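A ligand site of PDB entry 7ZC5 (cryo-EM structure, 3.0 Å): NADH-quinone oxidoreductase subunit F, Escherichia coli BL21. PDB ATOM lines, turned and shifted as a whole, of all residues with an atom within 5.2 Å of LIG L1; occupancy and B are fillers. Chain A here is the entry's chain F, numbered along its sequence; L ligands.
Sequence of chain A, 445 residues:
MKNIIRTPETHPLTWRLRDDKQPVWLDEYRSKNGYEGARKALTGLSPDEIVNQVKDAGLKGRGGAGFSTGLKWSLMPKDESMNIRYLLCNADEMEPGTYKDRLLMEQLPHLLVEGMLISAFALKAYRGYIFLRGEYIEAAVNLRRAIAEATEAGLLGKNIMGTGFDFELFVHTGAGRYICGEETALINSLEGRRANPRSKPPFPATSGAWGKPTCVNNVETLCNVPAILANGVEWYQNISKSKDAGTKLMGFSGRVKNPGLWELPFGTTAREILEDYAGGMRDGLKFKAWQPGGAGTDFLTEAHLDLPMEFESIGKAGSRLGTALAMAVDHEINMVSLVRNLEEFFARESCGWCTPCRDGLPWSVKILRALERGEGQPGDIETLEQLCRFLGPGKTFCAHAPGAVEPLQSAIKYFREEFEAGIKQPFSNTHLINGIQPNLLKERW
The side-chain amino group of Lys 72 lies within salt-bridge range of an oxygen (O8) of LG2 L2, 3.2 Å away. An oxygen (O5) of LIG L1 is in hydrogen-bond range of the side-chain amino group (NZ) of Lys 72, at 3.1 Å. The backbone NH (N) of Glu 93 lies within hydrogen-bond range of an oxygen (O2) of LG2 L2 (3.0 Å). O of Gly 64 sits at hydrogen-bond distance from O12 of LIG L1 (3.0 Å). The side-chain carboxylate (OE2) of Glu 183 lies within hydrogen-bond range of an oxygen (O6) of LIG L1 (2.6 Å). An oxygen (O7) of LG2 L2 sits at hydrogen-bond distance from the backbone NH (N) of Gly 63, at 3.0 Å. An oxygen (O13) of LIG L1 is in hydrogen-bond range of the guanidinium group (NH1) of Arg 320 (2.5 Å). N of Ala 65 is in hydrogen-bond range of O12 of LIG L1. O2 of LIG L1 is in salt-bridge range of NZ of Lys 200, 3.7 Å away.
An oxygen (O9) of LIG L1 is in hydrogen-bond range of an oxygen (O3) of LG2 L2, at 2.5 Å.
OH of Tyr 178 sits at hydrogen-bond distance from OE1 of Glu 95 (2.6 Å). The backbone NH of Thr 323 sits at hydrogen-bond distance from the backbone carbonyl oxygen of Gly 293. The side-chain hydroxyl (OG1) of Thr 98 is in hydrogen-bond range of the backbone carbonyl oxygen (O) of Glu 95 (3.2 Å). The side-chain amino group of Lys 200 is in salt-bridge range of the side-chain carboxylate of Glu 183, 3.2 Å away. The side-chain carboxylate of Glu 93 lies within hydrogen-bond range of the backbone NH of Lys 100 (2.9 Å).
The backbone carbonyl oxygen (O) of Gly 63 sits close to an oxygen (O14) of LIG L1 (3.4 Å). The side-chain carboxylate of Glu 182 sits close to an oxygen (O9) of LIG L1 (3.1 Å). Phe 67 touches LIG L1. CD2 of Leu 75 touches C9 of LIG L1, 3.5 Å away. CA of Glu 93 touches N7 of LIG L1, at 3.6 Å. Met 94 touches LIG L1. Glu 95 touches LIG L1 (CB to N7, 3.4 Å). Tyr 178 touches LIG L1. Phe 203 touches LIG L1 (CZ to C8, 3.4 Å). Gly 322 touches LIG L1 (CA to O13, 3.99 Å). Thr 323 touches LIG L1 (CG2 to O14, 3.4 Å). CB of Ala 399 touches O8 of LIG L1, 3.5 Å away. Hydrophobic or aromatic side chains within 4 Å of LIG L1: Ala 65, Phe 67, Leu 75, Tyr 178, Phe 203 and Ala 399. The nearest printed residue that does not touch LIG L1 is Val 216 (4.2 Å).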
ATOM      1  N   GLY A  63      -9.661  33.007  26.227  1.00  0.00           N
ATOM      2  CA  GLY A  63      -9.281  31.623  26.318  1.00  0.00           C
ATOM      3  C   GLY A  63      -7.795  31.386  26.276  1.00  0.00           C
ATOM      4  O   GLY A  63      -7.363  30.234  26.268  1.00  0.00           O
ATOM      5  N   GLY A  64      -6.983  32.442  26.253  1.00  0.00           N
ATOM      6  CA  GLY A  64      -5.555  32.278  26.297  1.00  0.00           C
ATOM      7  C   GLY A  64      -4.798  32.843  25.125  1.00  0.00           C
ATOM      8  O   GLY A  64      -3.718  33.421  25.290  1.00  0.00           O
ATOM      9  N   ALA A  65      -5.338  32.688  23.917  1.00  0.00           N
ATOM     10  CA  ALA A  65      -4.601  33.109  22.733  1.00  0.00           C
ATOM     11  C   ALA A  65      -4.704  34.596  22.464  1.00  0.00           C
ATOM     12  O   ALA A  65      -3.824  35.168  21.824  1.00  0.00           O
ATOM     13  CB  ALA A  65      -5.072  32.323  21.523  1.00  0.00           C
ATOM     14  N   PHE A  67      -6.885  36.286  20.602  1.00  0.00           N
ATOM     15  CA  PHE A  67      -7.389  36.708  19.306  1.00  0.00           C
ATOM     16  C   PHE A  67      -8.601  37.619  19.486  1.00  0.00           C
ATOM     17  O   PHE A  67      -9.384  37.463  20.422  1.00  0.00           O
ATOM     18  CB  PHE A  67      -7.761  35.499  18.459  1.00  0.00           C
ATOM     19  CG  PHE A  67      -7.817  35.768  16.981  1.00  0.00           C
ATOM     20  CD1 PHE A  67      -6.646  35.862  16.249  1.00  0.00           C
ATOM     21  CD2 PHE A  67      -9.022  35.929  16.338  1.00  0.00           C
ATOM     22  CE1 PHE A  67      -6.688  36.106  14.895  1.00  0.00           C
ATOM     23  CE2 PHE A  67      -9.065  36.181  14.978  1.00  0.00           C
ATOM     24  CZ  PHE A  67      -7.893  36.273  14.260  1.00  0.00           C
ATOM     25  N   LYS A  72     -12.939  37.558  14.705  1.00  0.00           N
ATOM     26  CA  LYS A  72     -13.429  36.190  14.571  1.00  0.00           C
ATOM     27  C   LYS A  72     -14.880  36.157  14.143  1.00  0.00           C
ATOM     28  O   LYS A  72     -15.284  35.296  13.353  1.00  0.00           O
ATOM     29  CB  LYS A  72     -13.250  35.440  15.897  1.00  0.00           C
ATOM     30  CG  LYS A  72     -12.330  34.268  15.808  1.00  0.00           C
ATOM     31  CD  LYS A  72     -12.050  33.690  17.171  1.00  0.00           C
ATOM     32  CE  LYS A  72     -13.263  33.023  17.722  1.00  0.00           C
ATOM     33  NZ  LYS A  72     -12.922  32.305  18.971  1.00  0.00           N
ATOM     34  N   LEU A  75     -15.530  36.969  10.352  1.00  0.00           N
ATOM     35  CA  LEU A  75     -15.055  35.994   9.381  1.00  0.00           C
ATOM     36  C   LEU A  75     -16.095  34.946   9.047  1.00  0.00           C
ATOM     37  O   LEU A  75     -15.797  34.024   8.266  1.00  0.00           O
ATOM     38  CB  LEU A  75     -13.774  35.330   9.888  1.00  0.00           C
ATOM     39  CG  LEU A  75     -12.461  35.869   9.322  1.00  0.00           C
ATOM     40  CD1 LEU A  75     -12.437  37.390   9.241  1.00  0.00           C
ATOM     41  CD2 LEU A  75     -11.312  35.382  10.161  1.00  0.00           C
ATOM     42  N   GLU A  93     -12.004  24.014  29.868  1.00  0.00           N
ATOM     43  CA  GLU A  93     -11.109  24.567  30.890  1.00  0.00           C
ATOM     44  C   GLU A  93     -10.355  23.468  31.639  1.00  0.00           C
ATOM     45  O   GLU A  93     -10.542  23.257  32.837  1.00  0.00           O
ATOM     46  CB  GLU A  93     -11.880  25.465  31.865  1.00  0.00           C
ATOM     47  CG  GLU A  93     -11.002  26.466  32.563  1.00  0.00           C
ATOM     48  CD  GLU A  93     -11.571  26.901  33.888  1.00  0.00           C
ATOM     49  OE1 GLU A  93     -12.074  26.032  34.638  1.00  0.00           O
ATOM     50  OE2 GLU A  93     -11.516  28.103  34.177  1.00  0.00           O
ATOM     51  N   MET A  94      -9.526  22.757  30.897  1.00  0.00           N
ATOM     52  CA  MET A  94      -8.808  21.631  31.449  1.00  0.00           C
ATOM     53  C   MET A  94      -7.368  21.967  31.808  1.00  0.00           C
ATOM     54  O   MET A  94      -6.631  21.083  32.246  1.00  0.00           O
ATOM     55  CB  MET A  94      -8.826  20.473  30.455  1.00  0.00           C
ATOM     56  CG  MET A  94     -10.004  19.541  30.544  1.00  0.00           C
ATOM     57  SD  MET A  94      -9.580  18.021  31.386  1.00  0.00           S
ATOM     58  CE  MET A  94     -11.208  17.434  31.783  1.00  0.00           C
ATOM     59  N   GLU A  95      -6.950  23.208  31.620  1.00  0.00           N
ATOM     60  CA  GLU A  95      -5.563  23.571  31.867  1.00  0.00           C
ATOM     61  C   GLU A  95      -5.275  23.574  33.357  1.00  0.00           C
ATOM     62  O   GLU A  95      -6.042  24.168  34.127  1.00  0.00           O
ATOM     63  CB  GLU A  95      -5.245  24.939  31.273  1.00  0.00           C
ATOM     64  CG  GLU A  95      -3.805  25.399  31.416  1.00  0.00           C
ATOM     65  CD  GLU A  95      -2.937  25.029  30.215  1.00  0.00           C
ATOM     66  OE1 GLU A  95      -3.028  23.888  29.718  1.00  0.00           O
ATOM     67  OE2 GLU A  95      -2.164  25.897  29.753  1.00  0.00           O
ATOM     68  N   THR A  98      -6.040  26.617  36.088  1.00  0.00           N
ATOM     69  CA  THR A  98      -7.106  27.446  35.546  1.00  0.00           C
ATOM     70  C   THR A  98      -8.422  27.068  36.209  1.00  0.00           C
ATOM     71  O   THR A  98      -8.842  25.909  36.138  1.00  0.00           O
ATOM     72  CB  THR A  98      -7.214  27.293  34.027  1.00  0.00           C
ATOM     73  OG1 THR A  98      -5.893  27.256  33.484  1.00  0.00           O
ATOM     74  CG2 THR A  98      -7.958  28.461  33.435  1.00  0.00           C
ATOM     75  N   LYS A 100     -11.141  29.787  36.452  1.00  0.00           N
ATOM     76  CA  LYS A 100     -12.000  30.967  36.340  1.00  0.00           C
ATOM     77  C   LYS A 100     -13.394  30.621  35.829  1.00  0.00           C
ATOM     78  O   LYS A 100     -14.397  31.164  36.318  1.00  0.00           O
ATOM     79  CB  LYS A 100     -11.355  32.000  35.425  1.00  0.00           C
ATOM     80  CG  LYS A 100     -10.500  31.406  34.326  1.00  0.00           C
ATOM     81  CD  LYS A 100     -10.346  32.365  33.170  1.00  0.00           C
ATOM     82  CE  LYS A 100      -9.765  31.661  31.964  1.00  0.00           C
ATOM     83  NZ  LYS A 100     -10.008  32.401  30.709  1.00  0.00           N
ATOM     84  N   TYR A 178      -8.236  16.590  27.934  1.00  0.00           N
ATOM     85  CA  TYR A 178      -7.733  17.959  27.885  1.00  0.00           C
ATOM     86  C   TYR A 178      -7.754  18.511  26.481  1.00  0.00           C
ATOM     87  O   TYR A 178      -8.009  19.702  26.272  1.00  0.00           O
ATOM     88  CB  TYR A 178      -6.318  17.989  28.462  1.00  0.00           C
ATOM     89  CG  TYR A 178      -5.505  19.233  28.193  1.00  0.00           C
ATOM     90  CD1 TYR A 178      -5.727  20.398  28.905  1.00  0.00           C
ATOM     91  CD2 TYR A 178      -4.488  19.230  27.257  1.00  0.00           C
ATOM     92  CE1 TYR A 178      -4.981  21.515  28.676  1.00  0.00           C
ATOM     93  CE2 TYR A 178      -3.741  20.346  27.029  1.00  0.00           C
ATOM     94  CZ  TYR A 178      -3.982  21.482  27.737  1.00  0.00           C
ATOM     95  OH  TYR A 178      -3.226  22.599  27.507  1.00  0.00           O
ATOM     96  N   GLU A 182      -9.319  22.225  22.763  1.00  0.00           N
ATOM     97  CA  GLU A 182      -8.912  22.724  21.459  1.00  0.00           C
ATOM     98  C   GLU A 182     -10.140  22.868  20.576  1.00  0.00           C
ATOM     99  O   GLU A 182     -10.953  21.942  20.486  1.00  0.00           O
ATOM    100  CB  GLU A 182      -7.923  21.763  20.816  1.00  0.00           C
ATOM    101  CG  GLU A 182      -6.759  22.401  20.142  1.00  0.00           C
ATOM    102  CD  GLU A 182      -7.067  22.922  18.771  1.00  0.00           C
ATOM    103  OE1 GLU A 182      -7.384  22.116  17.880  1.00  0.00           O
ATOM    104  OE2 GLU A 182      -6.972  24.143  18.551  1.00  0.00           O
ATOM    105  N   GLU A 183     -10.275  24.020  19.918  1.00  0.00           N
ATOM    106  CA  GLU A 183     -11.553  24.393  19.318  1.00  0.00           C
ATOM    107  C   GLU A 183     -11.945  23.459  18.179  1.00  0.00           C
ATOM    108  O   GLU A 183     -13.111  23.049  18.086  1.00  0.00           O
ATOM    109  CB  GLU A 183     -11.522  25.838  18.830  1.00  0.00           C
ATOM    110  CG  GLU A 183     -10.309  26.189  18.021  1.00  0.00           C
ATOM    111  CD  GLU A 183     -10.625  27.228  16.978  1.00  0.00           C
ATOM    112  OE1 GLU A 183     -11.622  27.964  17.157  1.00  0.00           O
ATOM    113  OE2 GLU A 183      -9.883  27.315  15.982  1.00  0.00           O
ATOM    114  N   LYS A 200      -6.039  23.946   9.979  1.00  0.00           N
ATOM    115  CA  LYS A 200      -6.650  25.210   9.594  1.00  0.00           C
ATOM    116  C   LYS A 200      -5.668  25.949   8.692  1.00  0.00           C
ATOM    117  O   LYS A 200      -4.472  25.999   9.000  1.00  0.00           O
ATOM    118  CB  LYS A 200      -6.987  26.052  10.828  1.00  0.00           C
ATOM    119  CG  LYS A 200      -7.938  25.387  11.799  1.00  0.00           C
ATOM    120  CD  LYS A 200      -8.021  26.152  13.097  1.00  0.00           C
ATOM    121  CE  LYS A 200      -6.703  26.105  13.851  1.00  0.00           C
ATOM    122  NZ  LYS A 200      -6.798  26.779  15.162  1.00  0.00           N
ATOM    123  N   PHE A 203     -10.871  27.399   8.599  1.00  0.00           N
ATOM    124  CA  PHE A 203     -11.185  27.731   9.969  1.00  0.00           C
ATOM    125  C   PHE A 203     -12.630  27.384  10.269  1.00  0.00           C
ATOM    126  O   PHE A 203     -13.438  27.271   9.345  1.00  0.00           O
ATOM    127  CB  PHE A 203     -10.892  29.200  10.224  1.00  0.00           C
ATOM    128  CG  PHE A 203      -9.437  29.507  10.300  1.00  0.00           C
ATOM    129  CD1 PHE A 203      -8.741  29.315  11.481  1.00  0.00           C
ATOM    130  CD2 PHE A 203      -8.755  29.960   9.194  1.00  0.00           C
ATOM    131  CE1 PHE A 203      -7.394  29.581  11.553  1.00  0.00           C
ATOM    132  CE2 PHE A 203      -7.409  30.229   9.253  1.00  0.00           C
ATOM    133  CZ  PHE A 203      -6.723  30.036  10.435  1.00  0.00           C
ATOM    134  N   PRO A 204     -12.984  27.193  11.533  1.00  0.00           N
ATOM    135  CA  PRO A 204     -14.388  26.890  11.873  1.00  0.00           C
ATOM    136  C   PRO A 204     -15.367  27.997  11.514  1.00  0.00           C
ATOM    137  O   PRO A 204     -16.561  27.723  11.451  1.00  0.00           O
ATOM    138  CB  PRO A 204     -14.332  26.652  13.379  1.00  0.00           C
ATOM    139  CG  PRO A 204     -12.969  26.168  13.629  1.00  0.00           C
ATOM    140  CD  PRO A 204     -12.093  26.924  12.684  1.00  0.00           C
ATOM    141  N   VAL A 216     -16.364  29.319  17.986  1.00  0.00           N
ATOM    142  CA  VAL A 216     -15.994  28.834  19.306  1.00  0.00           C
ATOM    143  C   VAL A 216     -15.433  30.007  20.096  1.00  0.00           C
ATOM    144  O   VAL A 216     -14.502  30.679  19.651  1.00  0.00           O
ATOM    145  CB  VAL A 216     -14.956  27.705  19.219  1.00  0.00           C
ATOM    146  CG1 VAL A 216     -14.715  27.109  20.583  1.00  0.00           C
ATOM    147  CG2 VAL A 216     -15.421  26.637  18.258  1.00  0.00           C
ATOM    148  N   GLY A 293       0.304  32.061  33.099  1.00  0.00           N
ATOM    149  CA  GLY A 293      -1.004  31.733  32.560  1.00  0.00           C
ATOM    150  C   GLY A 293      -1.365  30.276  32.445  1.00  0.00           C
ATOM    151  O   GLY A 293      -2.054  29.894  31.491  1.00  0.00           O
ATOM    152  N   THR A 297       2.655  27.536  29.939  1.00  0.00           N
ATOM    153  CA  THR A 297       3.396  28.774  29.750  1.00  0.00           C
ATOM    154  C   THR A 297       4.794  28.675  30.354  1.00  0.00           C
ATOM    155  O   THR A 297       5.074  27.814  31.182  1.00  0.00           O
ATOM    156  CB  THR A 297       2.639  29.942  30.363  1.00  0.00           C
ATOM    157  OG1 THR A 297       2.242  29.605  31.691  1.00  0.00           O
ATOM    158  CG2 THR A 297       1.398  30.235  29.562  1.00  0.00           C
ATOM    159  N   ARG A 320       3.840  33.646  27.706  1.00  0.00           N
ATOM    160  CA  ARG A 320       2.539  34.105  27.241  1.00  0.00           C
ATOM    161  C   ARG A 320       1.674  34.425  28.440  1.00  0.00           C
ATOM    162  O   ARG A 320       1.817  33.826  29.509  1.00  0.00           O
ATOM    163  CB  ARG A 320       1.831  33.060  26.384  1.00  0.00           C
ATOM    164  CG  ARG A 320       2.733  32.199  25.546  1.00  0.00           C
ATOM    165  CD  ARG A 320       1.920  31.285  24.654  1.00  0.00           C
ATOM    166  NE  ARG A 320       1.688  29.979  25.251  1.00  0.00           N
ATOM    167  CZ  ARG A 320       0.647  29.672  25.998  1.00  0.00           C
ATOM    168  NH1 ARG A 320      -0.303  30.560  26.266  1.00  0.00           N
ATOM    169  NH2 ARG A 320       0.540  28.438  26.493  1.00  0.00           N
ATOM    170  N   GLY A 322      -1.510  33.845  28.602  1.00  0.00           N
ATOM    171  CA  GLY A 322      -2.291  32.637  28.809  1.00  0.00           C
ATOM    172  C   GLY A 322      -3.650  32.941  29.379  1.00  0.00           C
ATOM    173  O   GLY A 322      -4.337  33.885  28.983  1.00  0.00           O
ATOM    174  N   THR A 323      -4.054  32.132  30.361  1.00  0.00           N
ATOM    175  CA  THR A 323      -5.303  32.352  31.054  1.00  0.00           C
ATOM    176  C   THR A 323      -5.182  33.376  32.170  1.00  0.00           C
ATOM    177  O   THR A 323      -6.171  33.618  32.860  1.00  0.00           O
ATOM    178  CB  THR A 323      -5.830  31.043  31.619  1.00  0.00           C
ATOM    179  OG1 THR A 323      -5.013  30.621  32.719  1.00  0.00           O
ATOM    180  CG2 THR A 323      -5.801  29.962  30.547  1.00  0.00           C
ATOM    181  N   ALA A 399      -1.427  22.911  18.915  1.00  0.00           N
ATOM    182  CA  ALA A 399      -0.590  23.663  19.831  1.00  0.00           C
ATOM    183  C   ALA A 399      -0.535  23.044  21.218  1.00  0.00           C
ATOM    184  O   ALA A 399      -0.262  23.743  22.195  1.00  0.00           O
ATOM    185  CB  ALA A 399      -1.068  25.108  19.908  1.00  0.00           C
HETATM  186  P1  LIG L   1      -4.802  30.154  18.049  1.00  0.00           P
HETATM  187  O1  LIG L   1      -3.752  31.164  18.251  1.00  0.00           O
HETATM  188  O2  LIG L   1      -4.539  29.149  16.951  1.00  0.00           O
HETATM  189  O3  LIG L   1      -6.199  30.847  17.721  1.00  0.00           O
HETATM  190  C1  LIG L   1      -7.106  31.262  18.762  1.00  0.00           C
HETATM  191  C2  LIG L   1      -8.474  31.561  18.215  1.00  0.00           C
HETATM  192  O4  LIG L   1      -8.383  32.510  17.130  1.00  0.00           O
HETATM  193  C3  LIG L   1      -9.259  30.372  17.687  1.00  0.00           C
HETATM  194  O5  LIG L   1     -10.644  30.511  17.959  1.00  0.00           O
HETATM  195  C4  LIG L   1      -8.979  30.428  16.179  1.00  0.00           C
HETATM  196  O6  LIG L   1     -10.037  29.861  15.427  1.00  0.00           O
HETATM  197  C5  LIG L   1      -8.889  31.935  15.936  1.00  0.00           C
HETATM  198  N1  LIG L   1      -8.008  32.308  14.850  1.00  0.00           N
HETATM  199  C6  LIG L   1      -6.644  32.490  14.919  1.00  0.00           C
HETATM  200  N2  LIG L   1      -6.099  32.840  13.780  1.00  0.00           N
HETATM  201  C7  LIG L   1      -7.177  32.884  12.896  1.00  0.00           C
HETATM  202  C8  LIG L   1      -7.265  33.186  11.530  1.00  0.00           C
HETATM  203  N3  LIG L   1      -6.219  33.532  10.768  1.00  0.00           N
HETATM  204  N4  LIG L   1      -8.477  33.124  10.952  1.00  0.00           N
HETATM  205  C9  LIG L   1      -9.535  32.780  11.702  1.00  0.00           C
HETATM  206  N5  LIG L   1      -9.565  32.486  12.996  1.00  0.00           N
HETATM  207  C10 LIG L   1      -8.347  32.554  13.545  1.00  0.00           C
HETATM  208  O7  LIG L   1      -5.121  29.345  19.377  1.00  0.00           O
HETATM  209  P2  LIG L   1      -5.060  27.804  19.792  1.00  0.00           P
HETATM  210  O8  LIG L   1      -3.750  27.266  19.261  1.00  0.00           O
HETATM  211  O9  LIG L   1      -6.263  27.067  19.378  1.00  0.00           O
HETATM  212  O10 LIG L   1      -4.924  27.800  21.378  1.00  0.00           O
HETATM  213  C11 LIG L   1      -3.682  28.006  22.074  1.00  0.00           C
HETATM  214  C12 LIG L   1      -3.948  28.974  23.209  1.00  0.00           C
HETATM  215  O11 LIG L   1      -4.911  28.386  24.117  1.00  0.00           O
HETATM  216  C13 LIG L   1      -2.727  29.367  24.046  1.00  0.00           C
HETATM  217  O12 LIG L   1      -2.657  30.771  24.234  1.00  0.00           O
HETATM  218  C14 LIG L   1      -2.963  28.642  25.373  1.00  0.00           C
HETATM  219  O13 LIG L   1      -2.481  29.415  26.471  1.00  0.00           O
HETATM  220  C15 LIG L   1      -4.483  28.576  25.440  1.00  0.00           C
HETATM  221  N6  LIG L   1      -4.961  27.454  26.238  1.00  0.00           N
HETATM  222  C16 LIG L   1      -6.004  27.633  27.154  1.00  0.00           C
HETATM  223  C17 LIG L   1      -6.485  26.633  27.918  1.00  0.00           C
HETATM  224  C18 LIG L   1      -7.600  26.954  28.827  1.00  0.00           C
HETATM  225  O14 LIG L   1      -8.089  28.084  28.851  1.00  0.00           O
HETATM  226  N7  LIG L   1      -8.051  25.987  29.616  1.00  0.00           N
HETATM  227  C19 LIG L   1      -5.914  25.251  27.806  1.00  0.00           C
HETATM  228  C20 LIG L   1      -4.805  25.188  26.833  1.00  0.00           C
HETATM  229  C21 LIG L   1      -4.403  26.223  26.121  1.00  0.00           C
HETATM  230  N1  LG2 L   2      -9.739  27.221  25.229  1.00  0.00           N
HETATM  231  C1  LG2 L   2     -10.707  27.161  26.205  1.00  0.00           C
HETATM  232  O1  LG2 L   2     -11.465  28.112  26.326  1.00  0.00           O
HETATM  233  N2  LG2 L   2     -10.803  26.071  27.024  1.00  0.00           N
HETATM  234  C2  LG2 L   2      -9.931  25.022  26.856  1.00  0.00           C
HETATM  235  O2  LG2 L   2     -10.014  24.044  27.587  1.00  0.00           O
HETATM  236  C3  LG2 L   2      -8.962  25.073  25.886  1.00  0.00           C
HETATM  237  N3  LG2 L   2      -8.100  24.028  25.727  1.00  0.00           N
HETATM  238  C4  LG2 L   2      -7.151  24.073  24.750  1.00  0.00           C
HETATM  239  C5  LG2 L   2      -6.285  23.003  24.607  1.00  0.00           C
HETATM  240  C6  LG2 L   2      -5.305  23.033  23.639  1.00  0.00           C
HETATM  241  C7  LG2 L   2      -4.381  21.873  23.494  1.00  0.00           C
HETATM  242  C8  LG2 L   2      -5.200  24.132  22.813  1.00  0.00           C
HETATM  243  C9  LG2 L   2      -4.139  24.177  21.758  1.00  0.00           C
HETATM  244  C10 LG2 L   2      -6.068  25.204  22.942  1.00  0.00           C
HETATM  245  C11 LG2 L   2      -7.048  25.180  23.919  1.00  0.00           C
HETATM  246  N4  LG2 L   2      -7.921  26.238  24.081  1.00  0.00           N
HETATM  247  C12 LG2 L   2      -8.867  26.171  25.061  1.00  0.00           C
HETATM  248  C13 LG2 L   2      -7.882  27.465  23.209  1.00  0.00           C
HETATM  249  C14 LG2 L   2      -8.879  27.295  22.056  1.00  0.00           C
HETATM  250  O3  LG2 L   2      -8.217  26.725  20.962  1.00  0.00           O
HETATM  251  C15 LG2 L   2      -9.501  28.608  21.602  1.00  0.00           C
HETATM  252  O4  LG2 L   2      -8.468  29.554  21.475  1.00  0.00           O
HETATM  253  C16 LG2 L   2     -10.529  29.103  22.607  1.00  0.00           C
HETATM  254  O5  LG2 L   2     -11.204  28.010  23.166  1.00  0.00           O
HETATM  255  C17 LG2 L   2     -11.558  30.057  22.028  1.00  0.00           C
HETATM  256  O6  LG2 L   2     -10.957  31.260  21.616  1.00  0.00           O
HETATM  257  P1  LG2 L   2     -11.246  32.620  22.416  1.00  0.00           P
HETATM  258  O7  LG2 L   2     -10.060  32.865  23.294  1.00  0.00           O
HETATM  259  O8  LG2 L   2     -11.440  33.763  21.467  1.00  0.00           O
HETATM  260  O9  LG2 L   2     -12.472  32.471  23.259  1.00  0.00           O
